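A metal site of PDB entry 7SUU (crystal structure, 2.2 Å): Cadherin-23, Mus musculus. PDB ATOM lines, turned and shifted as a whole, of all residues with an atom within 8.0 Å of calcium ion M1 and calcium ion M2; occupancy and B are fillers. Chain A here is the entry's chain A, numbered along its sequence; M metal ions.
The backbone carbonyl oxygen (O) of Ile 240 is bound to calcium ion M2, 2.3 Å away.
OD1 of Asp 239 is bound to calcium ion M2, 2.4 Å away.
Calcium ion M2 is bound by OD1 of Asp 242, at 2.4 Å.
Calcium ion M2 is bound by OE2 of Glu 140.
OE1 of Glu 195 is bound to calcium ion M2.
Slightly farther from calcium ion M2 lies OE2 of Glu 195 (3.0 Å).
Of the 14 residues printed, 5 come within 4 Å of calcium ion M1.
Along chain A the residues within 4 Å of calcium ion M1 span positions 140 to 242.
Calcium ion M1 is bound by OD2 of Asp 242 (2.0 Å), OD1 of Asp 193 (2.2 Å), OE2 of Glu 195 (2.3 Å), OE1 of Glu 140 (2.6 Å) and NE2 of His 141 (2.6 Å).
Calcium ion M1 has five donor atoms within binding distance.
O of Glu 238 lies within hydrogen-bond range of N of Glu 140 (3.2 Å).
OD1 of Asp 239 sits close to NE of Arg 194, at 3.6 Å.
The side-chain hydroxyl (OG1) of Thr 196 is in hydrogen-bond range of the side-chain carboxylate (OD2) of Asp 193 (2.5 Å).
OD1 of Asp 191 lies within hydrogen-bond range of ND1 of His 141, 2.9 Å away.
O of Leu 192 is in hydrogen-bond range of N of His 141 (2.6 Å).
OE1 of Glu 140 sits close to N of Arg 194 (2.6 Å).
Five residues have an atom within 4 Å of calcium ion M2: Glu 140, Glu 195, Asp 239, Ile 240 and Asp 242.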
ATOM      1  N   GLU A 140     -16.003  10.633  13.440  1.00  0.00           N
ATOM      2  CA  GLU A 140     -15.248  11.437  12.431  1.00  0.00           C
ATOM      3  C   GLU A 140     -13.929  11.902  13.059  1.00  0.00           C
ATOM      4  O   GLU A 140     -13.912  12.122  14.272  1.00  0.00           O
ATOM      5  CB  GLU A 140     -16.072  12.652  11.977  1.00  0.00           C
ATOM      6  CG  GLU A 140     -16.536  13.569  13.110  1.00  0.00           C
ATOM      7  CD  GLU A 140     -17.120  14.907  12.630  1.00  0.00           C
ATOM      8  OE1 GLU A 140     -16.919  15.252  11.456  1.00  0.00           O
ATOM      9  OE2 GLU A 140     -17.809  15.565  13.419  1.00  0.00           O
ATOM     10  N   HIS A 141     -12.891  12.106  12.255  1.00  0.00           N
ATOM     11  CA  HIS A 141     -11.589  12.657  12.731  1.00  0.00           C
ATOM     12  C   HIS A 141     -10.859  11.667  13.649  1.00  0.00           C
ATOM     13  O   HIS A 141      -9.907  12.076  14.303  1.00  0.00           O
ATOM     14  CB  HIS A 141     -11.809  14.052  13.354  1.00  0.00           C
ATOM     15  CG  HIS A 141     -12.460  15.042  12.423  1.00  0.00           C
ATOM     16  ND1 HIS A 141     -11.914  15.380  11.190  1.00  0.00           N
ATOM     17  CD2 HIS A 141     -13.597  15.756  12.524  1.00  0.00           C
ATOM     18  CE1 HIS A 141     -12.685  16.254  10.575  1.00  0.00           C
ATOM     19  NE2 HIS A 141     -13.712  16.527  11.379  1.00  0.00           N
ATOM     20  N   ASP A 191      -8.300  11.070   7.108  1.00  0.00           N
ATOM     21  CA  ASP A 191      -9.057  12.022   7.963  1.00  0.00           C
ATOM     22  C   ASP A 191     -10.499  12.053   7.456  1.00  0.00           C
ATOM     23  O   ASP A 191     -10.704  12.453   6.304  1.00  0.00           O
ATOM     24  CB  ASP A 191      -8.433  13.413   7.934  1.00  0.00           C
ATOM     25  CG  ASP A 191      -9.248  14.400   8.764  1.00  0.00           C
ATOM     26  OD1 ASP A 191      -9.781  13.983   9.830  1.00  0.00           O
ATOM     27  OD2 ASP A 191      -9.350  15.578   8.336  1.00  0.00           O
ATOM     28  N   LEU A 192     -11.454  11.620   8.265  1.00  0.00           N
ATOM     29  CA  LEU A 192     -12.864  11.553   7.816  1.00  0.00           C
ATOM     30  C   LEU A 192     -13.660  12.633   8.544  1.00  0.00           C
ATOM     31  O   LEU A 192     -13.524  12.773   9.796  1.00  0.00           O
ATOM     32  CB  LEU A 192     -13.410  10.140   8.046  1.00  0.00           C
ATOM     33  CG  LEU A 192     -12.582   9.019   7.411  1.00  0.00           C
ATOM     34  CD1 LEU A 192     -13.273   7.690   7.613  1.00  0.00           C
ATOM     35  CD2 LEU A 192     -12.309   9.275   5.935  1.00  0.00           C
ATOM     36  N   ASP A 193     -14.414  13.407   7.762  1.00  0.00           N
ATOM     37  CA  ASP A 193     -15.122  14.637   8.194  1.00  0.00           C
ATOM     38  C   ASP A 193     -16.618  14.463   7.934  1.00  0.00           C
ATOM     39  O   ASP A 193     -16.988  14.233   6.765  1.00  0.00           O
ATOM     40  CB  ASP A 193     -14.538  15.862   7.483  1.00  0.00           C
ATOM     41  CG  ASP A 193     -15.363  17.100   7.776  1.00  0.00           C
ATOM     42  OD1 ASP A 193     -15.880  17.214   8.929  1.00  0.00           O
ATOM     43  OD2 ASP A 193     -15.525  17.918   6.842  1.00  0.00           O
ATOM     44  N   ARG A 194     -17.429  14.519   8.991  1.00  0.00           N
ATOM     45  CA  ARG A 194     -18.899  14.259   8.922  1.00  0.00           C
ATOM     46  C   ARG A 194     -19.544  15.354   8.081  1.00  0.00           C
ATOM     47  O   ARG A 194     -20.483  15.069   7.334  1.00  0.00           O
ATOM     48  CB  ARG A 194     -19.533  14.272  10.320  1.00  0.00           C
ATOM     49  CG  ARG A 194     -21.033  13.948  10.352  1.00  0.00           C
ATOM     50  CD  ARG A 194     -21.541  14.015  11.774  1.00  0.00           C
ATOM     51  NE  ARG A 194     -22.982  14.127  11.902  1.00  0.00           N
ATOM     52  CZ  ARG A 194     -23.819  13.144  12.261  1.00  0.00           C
ATOM     53  NH1 ARG A 194     -23.400  11.910  12.484  1.00  0.00           N
ATOM     54  NH2 ARG A 194     -25.121  13.415  12.367  1.00  0.00           N
ATOM     55  N   GLU A 195     -19.034  16.575   8.176  1.00  0.00           N
ATOM     56  CA  GLU A 195     -19.620  17.772   7.534  1.00  0.00           C
ATOM     57  C   GLU A 195     -19.236  17.836   6.044  1.00  0.00           C
ATOM     58  O   GLU A 195     -19.643  18.823   5.428  1.00  0.00           O
ATOM     59  CB  GLU A 195     -19.198  19.024   8.312  1.00  0.00           C
ATOM     60  CG  GLU A 195     -19.922  19.168   9.648  1.00  0.00           C
ATOM     61  CD  GLU A 195     -19.521  18.213  10.768  1.00  0.00           C
ATOM     62  OE1 GLU A 195     -20.444  17.651  11.421  1.00  0.00           O
ATOM     63  OE2 GLU A 195     -18.287  18.074  11.032  1.00  0.00           O
ATOM     64  N   THR A 196     -18.570  16.821   5.482  1.00  0.00           N
ATOM     65  CA  THR A 196     -18.161  16.781   4.054  1.00  0.00           C
ATOM     66  C   THR A 196     -18.644  15.490   3.387  1.00  0.00           C
ATOM     67  O   THR A 196     -19.272  15.581   2.318  1.00  0.00           O
ATOM     68  CB  THR A 196     -16.640  16.901   3.883  1.00  0.00           C
ATOM     69  OG1 THR A 196     -16.193  18.127   4.468  1.00  0.00           O
ATOM     70  CG2 THR A 196     -16.197  16.891   2.435  1.00  0.00           C
ATOM     71  N   LEU A 237     -20.241   8.197   9.851  1.00  0.00           N
ATOM     72  CA  LEU A 237     -19.408   8.935  10.830  1.00  0.00           C
ATOM     73  C   LEU A 237     -20.314   9.456  11.935  1.00  0.00           C
ATOM     74  O   LEU A 237     -21.257  10.129  11.617  1.00  0.00           O
ATOM     75  CB  LEU A 237     -18.654  10.095  10.145  1.00  0.00           C
ATOM     76  CG  LEU A 237     -17.847   9.669   8.911  1.00  0.00           C
ATOM     77  CD1 LEU A 237     -16.979  10.796   8.348  1.00  0.00           C
ATOM     78  CD2 LEU A 237     -16.993   8.460   9.229  1.00  0.00           C
ATOM     79  N   GLU A 238     -19.994   9.128  13.190  1.00  0.00           N
ATOM     80  CA  GLU A 238     -20.643   9.689  14.398  1.00  0.00           C
ATOM     81  C   GLU A 238     -20.170  11.141  14.545  1.00  0.00           C
ATOM     82  O   GLU A 238     -18.965  11.426  14.294  1.00  0.00           O
ATOM     83  CB  GLU A 238     -20.289   8.905  15.663  1.00  0.00           C
ATOM     84  CG  GLU A 238     -20.704   7.442  15.625  1.00  0.00           C
ATOM     85  CD  GLU A 238     -20.105   6.646  16.775  1.00  0.00           C
ATOM     86  OE1 GLU A 238     -20.074   7.194  17.901  1.00  0.00           O
ATOM     87  OE2 GLU A 238     -19.641   5.503  16.544  1.00  0.00           O
ATOM     88  N   ASP A 239     -21.075  11.991  14.996  1.00  0.00           N
ATOM     89  CA  ASP A 239     -20.840  13.445  15.180  1.00  0.00           C
ATOM     90  C   ASP A 239     -19.863  13.658  16.331  1.00  0.00           C
ATOM     91  O   ASP A 239     -20.047  13.054  17.378  1.00  0.00           O
ATOM     92  CB  ASP A 239     -22.121  14.243  15.427  1.00  0.00           C
ATOM     93  CG  ASP A 239     -21.879  15.740  15.291  1.00  0.00           C
ATOM     94  OD1 ASP A 239     -21.244  16.142  14.328  1.00  0.00           O
ATOM     95  OD2 ASP A 239     -22.241  16.475  16.212  1.00  0.00           O
ATOM     96  N   ILE A 240     -18.841  14.462  16.079  1.00  0.00           N
ATOM     97  CA  ILE A 240     -17.991  15.159  17.078  1.00  0.00           C
ATOM     98  C   ILE A 240     -18.401  16.636  17.051  1.00  0.00           C
ATOM     99  O   ILE A 240     -18.768  17.158  15.948  1.00  0.00           O
ATOM    100  CB  ILE A 240     -16.499  14.911  16.764  1.00  0.00           C
ATOM    101  CG1 ILE A 240     -15.908  13.873  17.718  1.00  0.00           C
ATOM    102  CG2 ILE A 240     -15.653  16.163  16.763  1.00  0.00           C
ATOM    103  CD1 ILE A 240     -16.447  12.500  17.475  1.00  0.00           C
ATOM    104  N   ASN A 241     -18.333  17.282  18.210  1.00  0.00           N
ATOM    105  CA  ASN A 241     -18.580  18.748  18.324  1.00  0.00           C
ATOM    106  C   ASN A 241     -17.293  19.507  17.943  1.00  0.00           C
ATOM    107  O   ASN A 241     -16.513  19.835  18.850  1.00  0.00           O
ATOM    108  CB  ASN A 241     -19.133  19.064  19.710  1.00  0.00           C
ATOM    109  CG  ASN A 241     -19.729  20.446  19.791  1.00  0.00           C
ATOM    110  OD1 ASN A 241     -19.724  21.208  18.816  1.00  0.00           O
ATOM    111  ND2 ASN A 241     -20.230  20.796  20.972  1.00  0.00           N
ATOM    112  N   ASP A 242     -17.087  19.788  16.634  1.00  0.00           N
ATOM    113  CA  ASP A 242     -15.827  20.345  16.036  1.00  0.00           C
ATOM    114  C   ASP A 242     -16.106  21.720  15.418  1.00  0.00           C
ATOM    115  O   ASP A 242     -17.179  22.338  15.563  1.00  0.00           O
ATOM    116  CB  ASP A 242     -15.183  19.382  15.022  1.00  0.00           C
ATOM    117  CG  ASP A 242     -16.082  18.747  13.955  1.00  0.00           C
ATOM    118  OD1 ASP A 242     -17.318  18.733  14.106  1.00  0.00           O
ATOM    119  OD2 ASP A 242     -15.530  18.257  12.953  1.00  0.00           O
HETATM  120 CA    CA M   1     -16.070  17.698  11.111  1.00  0.00          CA
HETATM  121 CA    CA M   2     -19.360  17.496  13.772  1.00  0.00          CA
